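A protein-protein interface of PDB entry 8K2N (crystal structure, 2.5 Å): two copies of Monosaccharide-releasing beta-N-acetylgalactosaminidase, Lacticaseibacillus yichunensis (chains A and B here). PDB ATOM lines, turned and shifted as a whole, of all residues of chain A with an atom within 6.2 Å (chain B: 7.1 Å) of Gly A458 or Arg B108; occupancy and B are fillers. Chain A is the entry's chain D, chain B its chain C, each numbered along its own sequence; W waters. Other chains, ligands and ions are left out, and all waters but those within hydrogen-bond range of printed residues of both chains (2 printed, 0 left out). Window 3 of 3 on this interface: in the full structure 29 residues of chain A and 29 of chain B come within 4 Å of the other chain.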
ATOM      1  N   GLN A  77      -6.165  -2.196  -8.606  1.00  0.00           N
ATOM      2  CA  GLN A  77      -6.939  -2.244  -9.843  1.00  0.00           C
ATOM      3  C   GLN A  77      -6.107  -1.898 -11.096  1.00  0.00           C
ATOM      4  O   GLN A  77      -6.576  -1.917 -12.217  1.00  0.00           O
ATOM      5  CB  GLN A  77      -8.107  -1.268  -9.661  1.00  0.00           C
ATOM      6  CG  GLN A  77      -9.109  -1.747  -8.604  1.00  0.00           C
ATOM      7  CD  GLN A  77     -10.159  -2.689  -9.144  1.00  0.00           C
ATOM      8  OE1 GLN A  77     -11.195  -2.337  -9.739  1.00  0.00           O
ATOM      9  NE2 GLN A  77      -9.877  -3.956  -8.898  1.00  0.00           N
ATOM     10  N   LEU A  78      -4.843  -1.572 -10.945  1.00  0.00           N
ATOM     11  CA  LEU A  78      -3.980  -1.301 -12.085  1.00  0.00           C
ATOM     12  C   LEU A  78      -2.548  -1.627 -11.672  1.00  0.00           C
ATOM     13  O   LEU A  78      -1.749  -0.761 -11.321  1.00  0.00           O
ATOM     14  CB  LEU A  78      -4.110   0.160 -12.516  1.00  0.00           C
ATOM     15  CG  LEU A  78      -3.401   0.545 -13.819  1.00  0.00           C
ATOM     16  CD1 LEU A  78      -4.096  -0.105 -15.000  1.00  0.00           C
ATOM     17  CD2 LEU A  78      -3.374   2.051 -14.041  1.00  0.00           C
ATOM     18  N   GLN A 442      -5.371  10.887 -10.042  1.00  0.00           N
ATOM     19  CA  GLN A 442      -4.608  11.654 -11.034  1.00  0.00           C
ATOM     20  C   GLN A 442      -5.176  13.082 -11.148  1.00  0.00           C
ATOM     21  O   GLN A 442      -6.413  13.273 -11.218  1.00  0.00           O
ATOM     22  CB  GLN A 442      -4.701  10.941 -12.381  1.00  0.00           C
ATOM     23  CG  GLN A 442      -4.066  11.679 -13.562  1.00  0.00           C
ATOM     24  CD  GLN A 442      -4.098  10.818 -14.812  1.00  0.00           C
ATOM     25  OE1 GLN A 442      -5.107  10.178 -15.097  1.00  0.00           O
ATOM     26  NE2 GLN A 442      -2.980  10.695 -15.513  1.00  0.00           N
ATOM     27  N   VAL A 453      -7.590   2.205  -2.504  1.00  0.00           N
ATOM     28  CA  VAL A 453      -7.124   2.631  -3.823  1.00  0.00           C
ATOM     29  C   VAL A 453      -5.658   3.003  -3.740  1.00  0.00           C
ATOM     30  O   VAL A 453      -5.286   3.968  -3.072  1.00  0.00           O
ATOM     31  CB  VAL A 453      -7.947   3.818  -4.354  1.00  0.00           C
ATOM     32  CG1 VAL A 453      -7.415   4.411  -5.662  1.00  0.00           C
ATOM     33  CG2 VAL A 453      -9.398   3.359  -4.489  1.00  0.00           C
ATOM     34  N   ASP A 455      -3.738   3.075  -6.855  1.00  0.00           N
ATOM     35  CA  ASP A 455      -3.437   3.268  -8.289  1.00  0.00           C
ATOM     36  C   ASP A 455      -3.878   4.674  -8.765  1.00  0.00           C
ATOM     37  O   ASP A 455      -3.939   4.966  -9.948  1.00  0.00           O
ATOM     38  CB  ASP A 455      -4.066   2.140  -9.131  1.00  0.00           C
ATOM     39  CG  ASP A 455      -5.509   1.842  -8.753  1.00  0.00           C
ATOM     40  OD1 ASP A 455      -6.275   2.849  -8.851  1.00  0.00           O
ATOM     41  OD2 ASP A 455      -5.855   0.649  -8.174  1.00  0.00           O
ATOM     42  N   ALA A 456      -4.116   5.600  -7.827  1.00  0.00           N
ATOM     43  CA  ALA A 456      -4.478   6.992  -8.139  1.00  0.00           C
ATOM     44  C   ALA A 456      -5.768   7.044  -8.955  1.00  0.00           C
ATOM     45  O   ALA A 456      -5.903   7.926  -9.811  1.00  0.00           O
ATOM     46  CB  ALA A 456      -3.362   7.762  -8.820  1.00  0.00           C
ATOM     47  N   GLY A 457      -6.720   6.135  -8.640  1.00  0.00           N
ATOM     48  CA  GLY A 457      -8.009   6.117  -9.301  1.00  0.00           C
ATOM     49  C   GLY A 457      -7.905   5.489 -10.689  1.00  0.00           C
ATOM     50  O   GLY A 457      -8.618   5.851 -11.596  1.00  0.00           O
ATOM     51  N   GLY A 458      -7.037   4.514 -10.874  1.00  0.00           N
ATOM     52  CA  GLY A 458      -6.963   3.764 -12.127  1.00  0.00           C
ATOM     53  C   GLY A 458      -6.073   4.447 -13.175  1.00  0.00           C
ATOM     54  O   GLY A 458      -6.193   4.180 -14.369  1.00  0.00           O
ATOM     55  N   ALA A 459      -5.099   5.251 -12.727  1.00  0.00           N
ATOM     56  CA  ALA A 459      -4.271   6.044 -13.628  1.00  0.00           C
ATOM     57  C   ALA A 459      -2.815   5.576 -13.528  1.00  0.00           C
ATOM     58  O   ALA A 459      -2.146   5.559 -14.546  1.00  0.00           O
ATOM     59  CB  ALA A 459      -4.423   7.522 -13.320  1.00  0.00           C
ATOM     60  N   PHE A 460      -2.330   5.193 -12.327  1.00  0.00           N
ATOM     61  CA  PHE A 460      -0.916   4.893 -12.119  1.00  0.00           C
ATOM     62  C   PHE A 460      -0.774   3.474 -11.555  1.00  0.00           C
ATOM     63  O   PHE A 460      -1.583   3.051 -10.717  1.00  0.00           O
ATOM     64  CB  PHE A 460      -0.194   5.896 -11.210  1.00  0.00           C
ATOM     65  CG  PHE A 460      -0.342   7.362 -11.589  1.00  0.00           C
ATOM     66  CD1 PHE A 460      -0.146   7.793 -12.903  1.00  0.00           C
ATOM     67  CD2 PHE A 460      -0.667   8.315 -10.637  1.00  0.00           C
ATOM     68  CE1 PHE A 460      -0.366   9.112 -13.269  1.00  0.00           C
ATOM     69  CE2 PHE A 460      -0.903   9.627 -11.015  1.00  0.00           C
ATOM     70  CZ  PHE A 460      -0.781  10.023 -12.340  1.00  0.00           C
ATOM     71  N   TYR B  45     -17.298  -5.513 -20.308  1.00  0.00           N
ATOM     72  CA  TYR B  45     -16.524  -4.749 -21.292  1.00  0.00           C
ATOM     73  C   TYR B  45     -15.025  -4.727 -20.964  1.00  0.00           C
ATOM     74  O   TYR B  45     -14.568  -4.708 -19.814  1.00  0.00           O
ATOM     75  CB  TYR B  45     -17.036  -3.305 -21.448  1.00  0.00           C
ATOM     76  CG  TYR B  45     -16.965  -2.429 -20.224  1.00  0.00           C
ATOM     77  CD1 TYR B  45     -15.802  -1.734 -19.911  1.00  0.00           C
ATOM     78  CD2 TYR B  45     -18.053  -2.299 -19.368  1.00  0.00           C
ATOM     79  CE1 TYR B  45     -15.719  -0.946 -18.771  1.00  0.00           C
ATOM     80  CE2 TYR B  45     -17.988  -1.508 -18.230  1.00  0.00           C
ATOM     81  CZ  TYR B  45     -16.807  -0.843 -17.921  1.00  0.00           C
ATOM     82  OH  TYR B  45     -16.735  -0.067 -16.773  1.00  0.00           O
ATOM     83  N   GLN B  46     -14.276  -4.590 -22.053  1.00  0.00           N
ATOM     84  CA  GLN B  46     -12.829  -4.720 -22.094  1.00  0.00           C
ATOM     85  C   GLN B  46     -12.333  -4.192 -23.455  1.00  0.00           C
ATOM     86  O   GLN B  46     -13.034  -4.326 -24.468  1.00  0.00           O
ATOM     87  CB  GLN B  46     -12.505  -6.189 -21.804  1.00  0.00           C
ATOM     88  CG  GLN B  46     -11.373  -6.733 -22.640  1.00  0.00           C
ATOM     89  CD  GLN B  46     -10.893  -8.017 -22.050  1.00  0.00           C
ATOM     90  OE1 GLN B  46     -11.517  -9.052 -22.278  1.00  0.00           O
ATOM     91  NE2 GLN B  46      -9.822  -7.925 -21.273  1.00  0.00           N
ATOM     92  N   SER B  54      -3.603   2.837 -21.023  1.00  0.00           N
ATOM     93  CA  SER B  54      -4.177   1.773 -20.215  1.00  0.00           C
ATOM     94  C   SER B  54      -5.652   1.598 -20.543  1.00  0.00           C
ATOM     95  O   SER B  54      -6.090   0.482 -20.622  1.00  0.00           O
ATOM     96  CB  SER B  54      -3.945   2.024 -18.730  1.00  0.00           C
ATOM     97  OG  SER B  54      -2.553   1.908 -18.456  1.00  0.00           O
ATOM     98  N   PHE B  55      -6.366   2.667 -20.890  1.00  0.00           N
ATOM     99  CA  PHE B  55      -7.792   2.600 -21.194  1.00  0.00           C
ATOM    100  C   PHE B  55      -8.232   3.562 -22.318  1.00  0.00           C
ATOM    101  O   PHE B  55      -7.519   4.473 -22.689  1.00  0.00           O
ATOM    102  CB  PHE B  55      -8.597   2.961 -19.937  1.00  0.00           C
ATOM    103  CG  PHE B  55      -8.291   4.305 -19.317  1.00  0.00           C
ATOM    104  CD1 PHE B  55      -7.237   4.489 -18.413  1.00  0.00           C
ATOM    105  CD2 PHE B  55      -9.076   5.415 -19.618  1.00  0.00           C
ATOM    106  CE1 PHE B  55      -6.995   5.742 -17.834  1.00  0.00           C
ATOM    107  CE2 PHE B  55      -8.788   6.670 -19.081  1.00  0.00           C
ATOM    108  CZ  PHE B  55      -7.793   6.823 -18.149  1.00  0.00           C
ATOM    109  N   SER B  56      -9.477   3.406 -22.798  1.00  0.00           N
ATOM    110  CA  SER B  56     -10.075   4.236 -23.835  1.00  0.00           C
ATOM    111  C   SER B  56     -11.479   4.532 -23.359  1.00  0.00           C
ATOM    112  O   SER B  56     -12.182   3.632 -22.917  1.00  0.00           O
ATOM    113  CB  SER B  56     -10.061   3.517 -25.181  1.00  0.00           C
ATOM    114  OG  SER B  56      -8.695   3.156 -25.558  1.00  0.00           O
ATOM    115  N   GLU B  57     -11.819   5.800 -23.292  1.00  0.00           N
ATOM    116  CA  GLU B  57     -13.134   6.230 -22.871  1.00  0.00           C
ATOM    117  C   GLU B  57     -14.221   5.890 -23.890  1.00  0.00           C
ATOM    118  O   GLU B  57     -14.007   6.089 -25.080  1.00  0.00           O
ATOM    119  CB  GLU B  57     -13.109   7.736 -22.715  1.00  0.00           C
ATOM    120  CG  GLU B  57     -12.044   8.152 -21.739  1.00  0.00           C
ATOM    121  CD  GLU B  57     -12.372   9.489 -21.117  1.00  0.00           C
ATOM    122  OE1 GLU B  57     -12.838  10.342 -21.864  1.00  0.00           O
ATOM    123  OE2 GLU B  57     -12.173   9.658 -19.903  1.00  0.00           O
ATOM    124  N   LEU B  58     -15.360   5.354 -23.398  1.00  0.00           N
ATOM    125  CA  LEU B  58     -16.576   5.087 -24.176  1.00  0.00           C
ATOM    126  C   LEU B  58     -17.744   5.900 -23.611  1.00  0.00           C
ATOM    127  O   LEU B  58     -17.761   6.223 -22.411  1.00  0.00           O
ATOM    128  CB  LEU B  58     -16.954   3.597 -24.151  1.00  0.00           C
ATOM    129  CG  LEU B  58     -15.831   2.635 -24.501  1.00  0.00           C
ATOM    130  CD1 LEU B  58     -16.299   1.174 -24.535  1.00  0.00           C
ATOM    131  CD2 LEU B  58     -15.213   3.062 -25.813  1.00  0.00           C
ATOM    132  N   GLU B  70     -21.537   1.688 -12.315  1.00  0.00           N
ATOM    133  CA  GLU B  70     -20.357   0.852 -12.461  1.00  0.00           C
ATOM    134  C   GLU B  70     -20.234  -0.052 -11.247  1.00  0.00           C
ATOM    135  O   GLU B  70     -20.466   0.388 -10.087  1.00  0.00           O
ATOM    136  CB  GLU B  70     -19.103   1.686 -12.529  1.00  0.00           C
ATOM    137  CG  GLU B  70     -19.189   2.732 -13.610  1.00  0.00           C
ATOM    138  CD  GLU B  70     -17.915   3.516 -13.815  1.00  0.00           C
ATOM    139  OE1 GLU B  70     -17.170   3.654 -12.815  1.00  0.00           O
ATOM    140  OE2 GLU B  70     -17.635   3.891 -14.986  1.00  0.00           O
ATOM    141  N   LEU B 103     -22.950   6.052 -12.504  1.00  0.00           N
ATOM    142  CA  LEU B 103     -22.146   6.382 -13.674  1.00  0.00           C
ATOM    143  C   LEU B 103     -22.444   7.830 -14.062  1.00  0.00           C
ATOM    144  O   LEU B 103     -23.532   8.135 -14.493  1.00  0.00           O
ATOM    145  CB  LEU B 103     -22.445   5.446 -14.850  1.00  0.00           C
ATOM    146  CG  LEU B 103     -21.776   5.859 -16.172  1.00  0.00           C
ATOM    147  CD1 LEU B 103     -20.260   5.702 -16.089  1.00  0.00           C
ATOM    148  CD2 LEU B 103     -22.336   5.094 -17.378  1.00  0.00           C
ATOM    149  N   GLY B 105     -20.257   9.765 -16.013  1.00  0.00           N
ATOM    150  CA  GLY B 105     -19.523  10.263 -17.160  1.00  0.00           C
ATOM    151  C   GLY B 105     -19.198   9.181 -18.164  1.00  0.00           C
ATOM    152  O   GLY B 105     -19.928   8.236 -18.268  1.00  0.00           O
ATOM    153  N   PRO B 106     -18.130   9.279 -18.961  1.00  0.00           N
ATOM    154  CA  PRO B 106     -17.750   8.174 -19.854  1.00  0.00           C
ATOM    155  C   PRO B 106     -17.225   6.956 -19.094  1.00  0.00           C
ATOM    156  O   PRO B 106     -16.784   7.108 -17.964  1.00  0.00           O
ATOM    157  CB  PRO B 106     -16.613   8.765 -20.710  1.00  0.00           C
ATOM    158  CG  PRO B 106     -16.009   9.784 -19.757  1.00  0.00           C
ATOM    159  CD  PRO B 106     -17.202  10.413 -19.037  1.00  0.00           C
ATOM    160  N   VAL B 107     -17.280   5.769 -19.728  1.00  0.00           N
ATOM    161  CA  VAL B 107     -16.821   4.527 -19.121  1.00  0.00           C
ATOM    162  C   VAL B 107     -15.418   4.272 -19.660  1.00  0.00           C
ATOM    163  O   VAL B 107     -15.119   4.539 -20.813  1.00  0.00           O
ATOM    164  CB  VAL B 107     -17.781   3.313 -19.290  1.00  0.00           C
ATOM    165  CG1 VAL B 107     -19.172   3.710 -19.800  1.00  0.00           C
ATOM    166  CG2 VAL B 107     -17.224   2.212 -20.173  1.00  0.00           C
ATOM    167  N   ARG B 108     -14.550   3.759 -18.783  1.00  0.00           N
ATOM    168  CA  ARG B 108     -13.159   3.508 -19.107  1.00  0.00           C
ATOM    169  C   ARG B 108     -12.955   2.014 -19.351  1.00  0.00           C
ATOM    170  O   ARG B 108     -12.975   1.229 -18.405  1.00  0.00           O
ATOM    171  CB  ARG B 108     -12.311   4.015 -17.945  1.00  0.00           C
ATOM    172  CG  ARG B 108     -12.180   5.521 -17.909  1.00  0.00           C
ATOM    173  CD  ARG B 108     -11.572   5.804 -16.583  1.00  0.00           C
ATOM    174  NE  ARG B 108     -10.939   7.099 -16.436  1.00  0.00           N
ATOM    175  CZ  ARG B 108     -10.062   7.401 -15.462  1.00  0.00           C
ATOM    176  NH1 ARG B 108      -9.446   6.474 -14.726  1.00  0.00           N
ATOM    177  NH2 ARG B 108      -9.790   8.674 -15.259  1.00  0.00           N
ATOM    178  N   ALA B 109     -12.745   1.639 -20.617  1.00  0.00           N
ATOM    179  CA  ALA B 109     -12.467   0.270 -21.017  1.00  0.00           C
ATOM    180  C   ALA B 109     -10.980   0.090 -21.032  1.00  0.00           C
ATOM    181  O   ALA B 109     -10.339   0.753 -21.840  1.00  0.00           O
ATOM    182  CB  ALA B 109     -13.019  -0.032 -22.373  1.00  0.00           C
ATOM    183  N   TYR B 110     -10.517  -0.830 -20.172  1.00  0.00           N
ATOM    184  CA  TYR B 110      -9.115  -1.088 -19.913  1.00  0.00           C
ATOM    185  C   TYR B 110      -8.693  -2.312 -20.726  1.00  0.00           C
ATOM    186  O   TYR B 110      -9.492  -3.231 -20.925  1.00  0.00           O
ATOM    187  CB  TYR B 110      -8.819  -1.383 -18.416  1.00  0.00           C
ATOM    188  CG  TYR B 110      -8.767  -0.195 -17.501  1.00  0.00           C
ATOM    189  CD1 TYR B 110      -9.914   0.438 -17.155  1.00  0.00           C
ATOM    190  CD2 TYR B 110      -7.572   0.284 -16.993  1.00  0.00           C
ATOM    191  CE1 TYR B 110      -9.872   1.572 -16.362  1.00  0.00           C
ATOM    192  CE2 TYR B 110      -7.518   1.369 -16.141  1.00  0.00           C
ATOM    193  CZ  TYR B 110      -8.676   2.055 -15.845  1.00  0.00           C
ATOM    194  OH  TYR B 110      -8.733   3.243 -15.047  1.00  0.00           O
ATOM    195  N   GLN B 113      -8.175  -6.546 -18.518  1.00  0.00           N
ATOM    196  CA  GLN B 113      -9.061  -6.615 -17.364  1.00  0.00           C
ATOM    197  C   GLN B 113     -10.508  -6.294 -17.797  1.00  0.00           C
ATOM    198  O   GLN B 113     -10.793  -5.407 -18.654  1.00  0.00           O
ATOM    199  CB  GLN B 113      -8.568  -5.741 -16.180  1.00  0.00           C
ATOM    200  CG  GLN B 113      -8.911  -4.259 -16.245  1.00  0.00           C
ATOM    201  CD  GLN B 113      -8.663  -3.490 -14.966  1.00  0.00           C
ATOM    202  OE1 GLN B 113      -9.572  -3.070 -14.264  1.00  0.00           O
ATOM    203  NE2 GLN B 113      -7.408  -3.209 -14.676  1.00  0.00           N
ATOM    204  N   ARG B 115     -14.566  -5.399 -16.764  1.00  0.00           N
ATOM    205  CA  ARG B 115     -15.356  -4.522 -15.906  1.00  0.00           C
ATOM    206  C   ARG B 115     -16.825  -4.603 -16.355  1.00  0.00           C
ATOM    207  O   ARG B 115     -17.108  -4.960 -17.518  1.00  0.00           O
ATOM    208  CB  ARG B 115     -14.815  -3.076 -15.938  1.00  0.00           C
ATOM    209  CG  ARG B 115     -13.385  -2.949 -15.416  1.00  0.00           C
ATOM    210  CD  ARG B 115     -12.871  -1.528 -15.155  1.00  0.00           C
ATOM    211  NE  ARG B 115     -11.529  -1.492 -14.543  1.00  0.00           N
ATOM    212  CZ  ARG B 115     -11.125  -0.601 -13.649  1.00  0.00           C
ATOM    213  NH1 ARG B 115     -11.995   0.269 -13.200  1.00  0.00           N
ATOM    214  NH2 ARG B 115      -9.867  -0.570 -13.213  1.00  0.00           N
HETATM  215  O   HOH W   1     -10.516   4.242 -13.635  1.00  0.00           O
HETATM  216  O   HOH W   2     -11.180  -4.259 -11.888  1.00  0.00           O
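Of the printed residues of chain B, Gly A458 touches Phe B55 (3.9 Å), Arg B108 (3.996 Å) and Tyr B110 (2.8 Å).
Printed residues of chain A within 4 Å of Arg B108: Gly A457 and Gly A458.
Of chain B, only Arg B108 (3.3 Å) comes within 4 Å of Gly A457.
Of the printed residues of chain A, Phe B55 touches Gly A458 (3.9 Å).
Of the printed residues of chain A, Tyr B110 touches Leu A78 (3.9 Å) and Gly A458 (2.8 Å).
Ser B54 touches none of the printed residues of chain A.
The nearest printed residue of chain A that does not touch Arg B108 is Gln A442 (4.9 Å).
No position is printed for both chains.
Of the 7 pairs that touch across the chains among the printed residues, none has its exchanged pair printed and touching as well.
Water W1 lies within hydrogen-bond range of the side-chain hydroxyl of Tyr B110 (2.5 Å), the guanidinium group of Arg B108 (2.7 Å) and the backbone carbonyl oxygen of Gly A457 (3.2 Å).
Water W2 lies within hydrogen-bond range of OE1 of Gln A77 (2.9 Å) and OE1 of Gln B113 (3.1 Å).
The side-chain amide oxygen (OE1) of Gln B113 is in hydrogen-bond range of the guanidinium group (NE) of Arg B115, 2.5 Å away.
The guanidinium group (NH1) of Arg B108 lies within hydrogen-bond range of the side-chain hydroxyl (OH) of Tyr B110, at 3.3 Å.
The side-chain carboxylate (OD1) of Asp A455 is in hydrogen-bond range of the backbone NH (N) of Gly A458, 2.7 Å away.
The backbone NH of Gln A77 sits at hydrogen-bond distance from the side-chain carboxylate of Asp A455.
The backbone carbonyl oxygen (O) of Arg B115 lies within hydrogen-bond range of the backbone NH (N) of Tyr B45 (2.9 Å).
The side-chain amide nitrogen (NE2) of Gln B46 sits close to the backbone NH (N) of Gln B113.
Of the 10 printed residues of chain A, 4 touch a printed residue of chain B.
Printed residues of chain A that touch a printed residue of chain B: Gln A77, Leu A78, Gly A457 and Gly A458.
Hydrophobic or aromatic side chains of chain A that line the printed part of chain B: Leu A78.
Of the 17 printed residues of chain B, 5 touch a printed residue of chain A.
Hydrophobic or aromatic side chains of chain B that line the printed part of chain A: Phe B55 and Tyr B110.
Among the printed residues, 7 pairs touch across the chains.
The backbone carbonyl oxygen (O) of Gln A77 is in hydrogen-bond range of the side-chain amide nitrogen (NE2) of Gln B113.
The guanidinium group (NH1) of Arg B108 is in hydrogen-bond range of the backbone carbonyl oxygen (O) of Gly A457 (3.3 Å).
The backbone carbonyl oxygen (O) of Gly A458 lies within hydrogen-bond range of the side-chain hydroxyl (OH) of Tyr B110 (2.8 Å).
Arg B115 touches Gln A77.
Leu A78 touches Tyr B110.
Gly A458 touches Phe B55 (O to CE1, 3.9 Å).
Arg B108 touches Gly A458.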
